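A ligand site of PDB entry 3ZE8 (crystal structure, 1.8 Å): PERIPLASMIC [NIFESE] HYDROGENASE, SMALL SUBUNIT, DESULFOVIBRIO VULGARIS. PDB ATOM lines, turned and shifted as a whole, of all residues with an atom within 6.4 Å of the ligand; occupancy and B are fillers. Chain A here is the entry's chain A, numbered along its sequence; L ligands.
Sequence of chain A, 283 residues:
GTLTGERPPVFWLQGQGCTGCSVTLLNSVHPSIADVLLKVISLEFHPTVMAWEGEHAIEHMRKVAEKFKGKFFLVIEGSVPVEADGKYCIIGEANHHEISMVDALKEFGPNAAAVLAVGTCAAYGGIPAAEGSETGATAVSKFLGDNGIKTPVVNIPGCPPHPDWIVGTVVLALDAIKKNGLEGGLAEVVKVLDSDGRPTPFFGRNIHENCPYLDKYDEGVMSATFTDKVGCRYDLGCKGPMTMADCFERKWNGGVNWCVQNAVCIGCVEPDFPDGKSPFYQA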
ATOM      1  N   ILE A 207     -13.147  24.785 -23.670  1.00  0.00           N
ATOM      2  CA  ILE A 207     -13.211  23.430 -23.129  1.00  0.00           C
ATOM      3  C   ILE A 207     -11.824  22.921 -22.763  1.00  0.00           C
ATOM      4  O   ILE A 207     -11.589  22.461 -21.639  1.00  0.00           O
ATOM      5  CB  ILE A 207     -13.801  22.437 -24.158  1.00  0.00           C
ATOM      6  CG1 ILE A 207     -15.218  22.857 -24.568  1.00  0.00           C
ATOM      7  CG2 ILE A 207     -13.740  20.995 -23.630  1.00  0.00           C
ATOM      8  CD1 ILE A 207     -16.322  22.049 -23.955  1.00  0.00           C
ATOM      9  N   HIS A 208     -10.912  23.020 -23.728  1.00  0.00           N
ATOM     10  CA  HIS A 208      -9.540  22.501 -23.607  1.00  0.00           C
ATOM     11  C   HIS A 208      -8.793  23.096 -22.426  1.00  0.00           C
ATOM     12  O   HIS A 208      -8.125  22.369 -21.670  1.00  0.00           O
ATOM     13  CB  HIS A 208      -8.815  22.771 -24.926  1.00  0.00           C
ATOM     14  CG  HIS A 208      -7.370  22.372 -24.953  1.00  0.00           C
ATOM     15  ND1 HIS A 208      -6.964  21.054 -25.032  1.00  0.00           N
ATOM     16  CD2 HIS A 208      -6.236  23.111 -24.980  1.00  0.00           C
ATOM     17  CE1 HIS A 208      -5.645  21.009 -25.076  1.00  0.00           C
ATOM     18  NE2 HIS A 208      -5.175  22.244 -25.044  1.00  0.00           N
ATOM     19  N   GLU A 209      -8.884  24.412 -22.270  1.00  0.00           N
ATOM     20  CA  GLU A 209      -8.185  25.095 -21.181  1.00  0.00           C
ATOM     21  C   GLU A 209      -8.648  24.605 -19.815  1.00  0.00           C
ATOM     22  O   GLU A 209      -7.911  24.682 -18.838  1.00  0.00           O
ATOM     23  CB  GLU A 209      -8.374  26.616 -21.295  1.00  0.00           C
ATOM     24  CG  GLU A 209      -7.671  27.225 -22.498  1.00  0.00           C
ATOM     25  CD  GLU A 209      -7.988  28.712 -22.669  1.00  0.00           C
ATOM     26  OE1 GLU A 209      -8.596  29.304 -21.748  1.00  0.00           O
ATOM     27  OE2 GLU A 209      -7.634  29.275 -23.720  1.00  0.00           O
ATOM     28  N   CYS A 211      -9.960  21.372 -19.382  1.00  0.00           N
ATOM     29  CA  CYS A 211     -10.195  19.928 -19.526  1.00  0.00           C
ATOM     30  C   CYS A 211      -9.437  19.156 -18.459  1.00  0.00           C
ATOM     31  O   CYS A 211      -8.281  19.483 -18.178  1.00  0.00           O
ATOM     32  CB  CYS A 211      -9.766  19.436 -20.899  1.00  0.00           C
ATOM     33  SG  CYS A 211     -10.105  17.674 -21.197  1.00  0.00           S
ATOM     34  N   PRO A 212     -10.061  18.126 -17.870  1.00  0.00           N
ATOM     35  CA  PRO A 212      -9.344  17.299 -16.898  1.00  0.00           C
ATOM     36  C   PRO A 212      -8.189  16.487 -17.504  1.00  0.00           C
ATOM     37  O   PRO A 212      -7.404  15.906 -16.766  1.00  0.00           O
ATOM     38  CB  PRO A 212     -10.427  16.352 -16.393  1.00  0.00           C
ATOM     39  CG  PRO A 212     -11.430  16.305 -17.484  1.00  0.00           C
ATOM     40  CD  PRO A 212     -11.459  17.697 -18.037  1.00  0.00           C
ATOM     41  N   TYR A 213      -8.097  16.445 -18.821  1.00  0.00           N
ATOM     42  CA  TYR A 213      -7.036  15.695 -19.497  1.00  0.00           C
ATOM     43  C   TYR A 213      -5.931  16.588 -20.037  1.00  0.00           C
ATOM     44  O   TYR A 213      -5.026  16.108 -20.715  1.00  0.00           O
ATOM     45  CB  TYR A 213      -7.611  14.815 -20.615  1.00  0.00           C
ATOM     46  CG  TYR A 213      -8.719  13.927 -20.104  1.00  0.00           C
ATOM     47  CD1 TYR A 213      -8.453  12.883 -19.224  1.00  0.00           C
ATOM     48  CD2 TYR A 213     -10.035  14.149 -20.491  1.00  0.00           C
ATOM     49  CE1 TYR A 213      -9.478  12.094 -18.744  1.00  0.00           C
ATOM     50  CE2 TYR A 213     -11.047  13.364 -20.014  1.00  0.00           C
ATOM     51  CZ  TYR A 213     -10.773  12.341 -19.138  1.00  0.00           C
ATOM     52  OH  TYR A 213     -11.814  11.553 -18.683  1.00  0.00           O
ATOM     53  N   LEU A 214      -5.978  17.870 -19.690  1.00  0.00           N
ATOM     54  CA  LEU A 214      -5.007  18.841 -20.184  1.00  0.00           C
ATOM     55  C   LEU A 214      -3.580  18.473 -19.789  1.00  0.00           C
ATOM     56  O   LEU A 214      -2.644  18.676 -20.557  1.00  0.00           O
ATOM     57  CB  LEU A 214      -5.365  20.254 -19.699  1.00  0.00           C
ATOM     58  CG  LEU A 214      -4.481  21.398 -20.222  1.00  0.00           C
ATOM     59  CD1 LEU A 214      -4.485  21.447 -21.746  1.00  0.00           C
ATOM     60  CD2 LEU A 214      -4.907  22.740 -19.628  1.00  0.00           C
ATOM     61  N   ASP A 215      -3.415  17.924 -18.580  1.00  0.00           N
ATOM     62  CA  ASP A 215      -2.098  17.477 -18.145  1.00  0.00           C
ATOM     63  C   ASP A 215      -1.528  16.406 -19.084  1.00  0.00           C
ATOM     64  O   ASP A 215      -0.341  16.422 -19.411  1.00  0.00           O
ATOM     65  CB  ASP A 215      -2.101  17.020 -16.671  1.00  0.00           C
ATOM     66  CG  ASP A 215      -3.039  15.828 -16.413  1.00  0.00           C
ATOM     67  OD1 ASP A 215      -4.017  15.626 -17.167  1.00  0.00           O
ATOM     68  OD2 ASP A 215      -2.779  15.086 -15.437  1.00  0.00           O
ATOM     69  N   LYS A 216      -2.387  15.496 -19.544  1.00  0.00           N
ATOM     70  CA  LYS A 216      -1.972  14.466 -20.496  1.00  0.00           C
ATOM     71  C   LYS A 216      -1.626  15.058 -21.861  1.00  0.00           C
ATOM     72  O   LYS A 216      -0.668  14.638 -22.498  1.00  0.00           O
ATOM     73  CB  LYS A 216      -3.047  13.401 -20.649  1.00  0.00           C
ATOM     74  CG  LYS A 216      -3.388  12.678 -19.359  1.00  0.00           C
ATOM     75  CD  LYS A 216      -2.188  11.910 -18.833  1.00  0.00           C
ATOM     76  CE  LYS A 216      -2.538  11.141 -17.571  1.00  0.00           C
ATOM     77  NZ  LYS A 216      -1.379  10.365 -17.063  1.00  0.00           N
ATOM     78  N   TYR A 217      -2.448  16.002 -22.323  1.00  0.00           N
ATOM     79  CA  TYR A 217      -2.188  16.747 -23.551  1.00  0.00           C
ATOM     80  C   TYR A 217      -0.793  17.369 -23.471  1.00  0.00           C
ATOM     81  O   TYR A 217       0.017  17.247 -24.399  1.00  0.00           O
ATOM     82  CB  TYR A 217      -3.241  17.847 -23.707  1.00  0.00           C
ATOM     83  CG  TYR A 217      -3.039  18.780 -24.876  1.00  0.00           C
ATOM     84  CD1 TYR A 217      -3.550  18.486 -26.135  1.00  0.00           C
ATOM     85  CD2 TYR A 217      -2.352  19.988 -24.704  1.00  0.00           C
ATOM     86  CE1 TYR A 217      -3.383  19.353 -27.201  1.00  0.00           C
ATOM     87  CE2 TYR A 217      -2.180  20.863 -25.775  1.00  0.00           C
ATOM     88  CZ  TYR A 217      -2.684  20.540 -27.014  1.00  0.00           C
ATOM     89  OH  TYR A 217      -2.515  21.420 -28.063  1.00  0.00           O
ATOM     90  N   MET A 222      -1.269  10.461 -25.509  1.00  0.00           N
ATOM     91  CA  MET A 222      -2.501  10.402 -26.313  1.00  0.00           C
ATOM     92  C   MET A 222      -3.120   9.004 -26.352  1.00  0.00           C
ATOM     93  O   MET A 222      -2.433   8.024 -26.604  1.00  0.00           O
ATOM     94  CB  MET A 222      -2.193  10.787 -27.770  1.00  0.00           C
ATOM     95  CG  MET A 222      -1.694  12.202 -27.943  1.00  0.00           C
ATOM     96  SD  MET A 222      -2.950  13.351 -27.393  1.00  0.00           S
ATOM     97  CE  MET A 222      -1.962  14.843 -27.227  1.00  0.00           C
ATOM     98  N   GLY A 231      -5.495   8.729 -21.495  1.00  0.00           N
ATOM     99  CA  GLY A 231      -4.783   9.715 -22.307  1.00  0.00           C
ATOM    100  C   GLY A 231      -5.667  10.815 -22.838  1.00  0.00           C
ATOM    101  O   GLY A 231      -6.893  10.744 -22.758  1.00  0.00           O
ATOM    102  N   CYS A 232      -5.040  11.859 -23.374  1.00  0.00           N
ATOM    103  CA  CYS A 232      -5.747  12.937 -24.061  1.00  0.00           C
ATOM    104  C   CYS A 232      -6.391  12.388 -25.345  1.00  0.00           C
ATOM    105  O   CYS A 232      -5.856  11.450 -25.967  1.00  0.00           O
ATOM    106  CB  CYS A 232      -4.764  14.076 -24.356  1.00  0.00           C
ATOM    107  SG  CYS A 232      -5.358  15.367 -25.479  1.00  0.00           S
ATOM    108  N   ARG A 233      -7.526  12.959 -25.732  1.00  0.00           N
ATOM    109  CA  ARG A 233      -8.298  12.520 -26.906  1.00  0.00           C
ATOM    110  C   ARG A 233      -7.951  13.281 -28.214  1.00  0.00           C
ATOM    111  O   ARG A 233      -8.591  13.072 -29.243  1.00  0.00           O
ATOM    112  CB  ARG A 233      -9.801  12.681 -26.628  1.00  0.00           C
ATOM    113  CG  ARG A 233     -10.424  11.626 -25.690  1.00  0.00           C
ATOM    114  CD  ARG A 233     -10.024  11.794 -24.213  1.00  0.00           C
ATOM    115  NE  ARG A 233     -11.012  11.156 -23.331  1.00  0.00           N
ATOM    116  CZ  ARG A 233     -10.728  10.584 -22.160  1.00  0.00           C
ATOM    117  NH1 ARG A 233      -9.476  10.548 -21.738  1.00  0.00           N
ATOM    118  NH2 ARG A 233     -11.704  10.041 -21.429  1.00  0.00           N
ATOM    119  N   TYR A 234      -6.936  14.133 -28.158  1.00  0.00           N
ATOM    120  CA  TYR A 234      -6.558  14.959 -29.314  1.00  0.00           C
ATOM    121  C   TYR A 234      -6.317  14.177 -30.617  1.00  0.00           C
ATOM    122  O   TYR A 234      -6.838  14.539 -31.666  1.00  0.00           O
ATOM    123  CB  TYR A 234      -5.327  15.818 -28.956  1.00  0.00           C
ATOM    124  CG  TYR A 234      -4.851  16.687 -30.099  1.00  0.00           C
ATOM    125  CD1 TYR A 234      -5.408  17.940 -30.318  1.00  0.00           C
ATOM    126  CD2 TYR A 234      -3.837  16.261 -30.950  1.00  0.00           C
ATOM    127  CE1 TYR A 234      -4.967  18.737 -31.365  1.00  0.00           C
ATOM    128  CE2 TYR A 234      -3.390  17.048 -31.989  1.00  0.00           C
ATOM    129  CZ  TYR A 234      -3.954  18.292 -32.189  1.00  0.00           C
ATOM    130  OH  TYR A 234      -3.507  19.073 -33.236  1.00  0.00           O
ATOM    131  N   ASP A 235      -5.541  13.097 -30.542  1.00  0.00           N
ATOM    132  CA  ASP A 235      -5.294  12.281 -31.730  1.00  0.00           C
ATOM    133  C   ASP A 235      -6.547  11.596 -32.261  1.00  0.00           C
ATOM    134  O   ASP A 235      -6.658  11.320 -33.450  1.00  0.00           O
ATOM    135  CB  ASP A 235      -4.220  11.230 -31.448  1.00  0.00           C
ATOM    136  CG  ASP A 235      -2.825  11.797 -31.402  1.00  0.00           C
ATOM    137  OD1 ASP A 235      -2.618  12.991 -31.708  1.00  0.00           O
ATOM    138  OD2 ASP A 235      -1.908  11.023 -31.063  1.00  0.00           O
ATOM    139  N   CYS A 238     -10.458  15.066 -30.952  1.00  0.00           N
ATOM    140  CA  CYS A 238     -11.087  16.021 -30.023  1.00  0.00           C
ATOM    141  C   CYS A 238     -10.894  17.484 -30.449  1.00  0.00           C
ATOM    142  O   CYS A 238      -9.766  17.936 -30.683  1.00  0.00           O
ATOM    143  CB  CYS A 238     -10.559  15.818 -28.616  1.00  0.00           C
ATOM    144  SG  CYS A 238     -11.390  16.884 -27.384  1.00  0.00           S
ATOM    145  N   LYS A 239     -12.005  18.220 -30.547  1.00  0.00           N
ATOM    146  CA  LYS A 239     -11.968  19.626 -30.936  1.00  0.00           C
ATOM    147  C   LYS A 239     -12.125  20.598 -29.772  1.00  0.00           C
ATOM    148  O   LYS A 239     -12.347  21.795 -29.987  1.00  0.00           O
ATOM    149  CB  LYS A 239     -13.047  19.925 -31.989  1.00  0.00           C
ATOM    150  CG  LYS A 239     -12.947  19.080 -33.238  1.00  0.00           C
ATOM    151  CD  LYS A 239     -11.558  19.107 -33.836  1.00  0.00           C
ATOM    152  CE  LYS A 239     -11.499  18.400 -35.178  1.00  0.00           C
ATOM    153  NZ  LYS A 239     -12.152  17.070 -35.153  1.00  0.00           N
ATOM    154  N   GLY A 240     -12.015  20.093 -28.544  1.00  0.00           N
ATOM    155  CA  GLY A 240     -11.955  20.946 -27.372  1.00  0.00           C
ATOM    156  C   GLY A 240     -11.103  22.207 -27.478  1.00  0.00           C
ATOM    157  O   GLY A 240     -11.518  23.255 -26.985  1.00  0.00           O
ATOM    158  N   PRO A 241      -9.909  22.135 -28.117  1.00  0.00           N
ATOM    159  CA  PRO A 241      -9.074  23.330 -28.247  1.00  0.00           C
ATOM    160  C   PRO A 241      -9.729  24.515 -28.956  1.00  0.00           C
ATOM    161  O   PRO A 241      -9.332  25.654 -28.694  1.00  0.00           O
ATOM    162  CB  PRO A 241      -7.869  22.825 -29.057  1.00  0.00           C
ATOM    163  CG  PRO A 241      -7.717  21.412 -28.607  1.00  0.00           C
ATOM    164  CD  PRO A 241      -9.152  20.911 -28.475  1.00  0.00           C
ATOM    165  N   TRP A 258     -20.094  13.194 -20.313  1.00  0.00           N
ATOM    166  CA  TRP A 258     -19.951  14.278 -21.279  1.00  0.00           C
ATOM    167  C   TRP A 258     -19.061  13.806 -22.420  1.00  0.00           C
ATOM    168  O   TRP A 258     -18.410  12.759 -22.314  1.00  0.00           O
ATOM    169  CB  TRP A 258     -19.442  15.585 -20.633  1.00  0.00           C
ATOM    170  CG  TRP A 258     -18.000  15.603 -20.159  1.00  0.00           C
ATOM    171  CD1 TRP A 258     -17.443  14.810 -19.194  1.00  0.00           C
ATOM    172  CD2 TRP A 258     -16.977  16.519 -20.586  1.00  0.00           C
ATOM    173  NE1 TRP A 258     -16.116  15.155 -19.023  1.00  0.00           N
ATOM    174  CE2 TRP A 258     -15.810  16.200 -19.864  1.00  0.00           C
ATOM    175  CE3 TRP A 258     -16.929  17.560 -21.528  1.00  0.00           C
ATOM    176  CZ2 TRP A 258     -14.607  16.881 -20.039  1.00  0.00           C
ATOM    177  CZ3 TRP A 258     -15.736  18.250 -21.698  1.00  0.00           C
ATOM    178  CH2 TRP A 258     -14.593  17.906 -20.954  1.00  0.00           C
ATOM    179  N   VAL A 260     -16.224  14.522 -23.957  1.00  0.00           N
ATOM    180  CA  VAL A 260     -14.785  14.248 -23.866  1.00  0.00           C
ATOM    181  C   VAL A 260     -14.504  12.979 -23.051  1.00  0.00           C
ATOM    182  O   VAL A 260     -13.612  12.204 -23.383  1.00  0.00           O
ATOM    183  CB  VAL A 260     -14.001  15.468 -23.327  1.00  0.00           C
ATOM    184  CG1 VAL A 260     -12.541  15.110 -23.069  1.00  0.00           C
ATOM    185  CG2 VAL A 260     -14.103  16.637 -24.325  1.00  0.00           C
ATOM    186  N   CYS A 265     -14.868  15.658 -28.112  1.00  0.00           N
ATOM    187  CA  CYS A 265     -15.663  16.847 -28.425  1.00  0.00           C
ATOM    188  C   CYS A 265     -15.677  17.099 -29.942  1.00  0.00           C
ATOM    189  O   CYS A 265     -14.637  17.008 -30.599  1.00  0.00           O
ATOM    190  CB  CYS A 265     -15.103  18.080 -27.684  1.00  0.00           C
ATOM    191  SG  CYS A 265     -15.949  19.653 -28.065  1.00  0.00           S
HETATM  192 FE1  LIG L   1      -9.647  17.312 -25.846  1.00  0.00          FE
HETATM  193 FE2  LIG L   1      -7.897  19.222 -24.985  1.00  0.00          FE
HETATM  194 FE3  LIG L   1      -7.169  16.611 -24.854  1.00  0.00          FE
HETATM  195 FE4  LIG L   1      -9.118  17.592 -23.218  1.00  0.00          FE
HETATM  196  S1  LIG L   1      -6.898  18.169 -23.187  1.00  0.00           S
HETATM  197  S2  LIG L   1      -9.168  15.614 -24.375  1.00  0.00           S
HETATM  198  S3  LIG L   1     -10.138  19.165 -24.570  1.00  0.00           S
HETATM  199  S4  LIG L   1      -7.610  17.801 -26.781  1.00  0.00           S
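ND1 of His 208 binds FE2 of the ligand, 2.1 Å away.
SG of Cys 211 binds FE4 of the ligand, at 2.3 Å.
The side-chain sulfur (SG) of Cys 232 binds an iron atom (FE3) of the ligand, at 2.3 Å.
An iron atom (FE1) of the ligand is bound by the side-chain sulfur of Cys 238 (2.4 Å).
The backbone NH of Arg 233 sits close to a sulfur (S2) of the ligand.
The backbone NH (N) of Leu 214 sits close to a sulfur (S1) of the ligand, 3.6 Å away.
The backbone NH (N) of His 208 lies within hydrogen-bond range of the backbone carbonyl oxygen (O) of Gly 240, 3.3 Å away.
The side-chain sulfur (SG) of Cys 211 sits close to the backbone NH (N) of Tyr 213.
SG of Cys 232 lies close to N of Tyr 234, 3.3 Å away.
SG of Cys 232 lies close to SD of Met 222 (3.7 Å).
The backbone NH (N) of Cys 238 lies within hydrogen-bond range of the backbone carbonyl oxygen (O) of Arg 233 (3.2 Å).
SG of Cys 238 sits close to N of Gly 240 (3.5 Å).
The side-chain sulfur (SG) of Cys 238 sits close to the backbone NH (N) of Cys 265, 3.8 Å away.
The backbone carbonyl oxygen (O) of Val 260 is in hydrogen-bond range of the guanidinium group (NE) of Arg 233 (2.8 Å).
O of Tyr 213 lies close to S1 of the ligand, 3.7 Å away.
Residues that only touch the ligand: Val 260 (3.7 Å), Tyr 217 (3.7 Å), Tyr 234 (3.7 Å), Gly 240 (3.8 Å) and Pro 241 (3.9 Å).
Hydrophobic or aromatic side chains that line the ligand: His 208, Tyr 217, Tyr 234, Pro 241 and Val 260.
Along chain A the residues within 4 Å of the ligand span positions 208 to 260.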
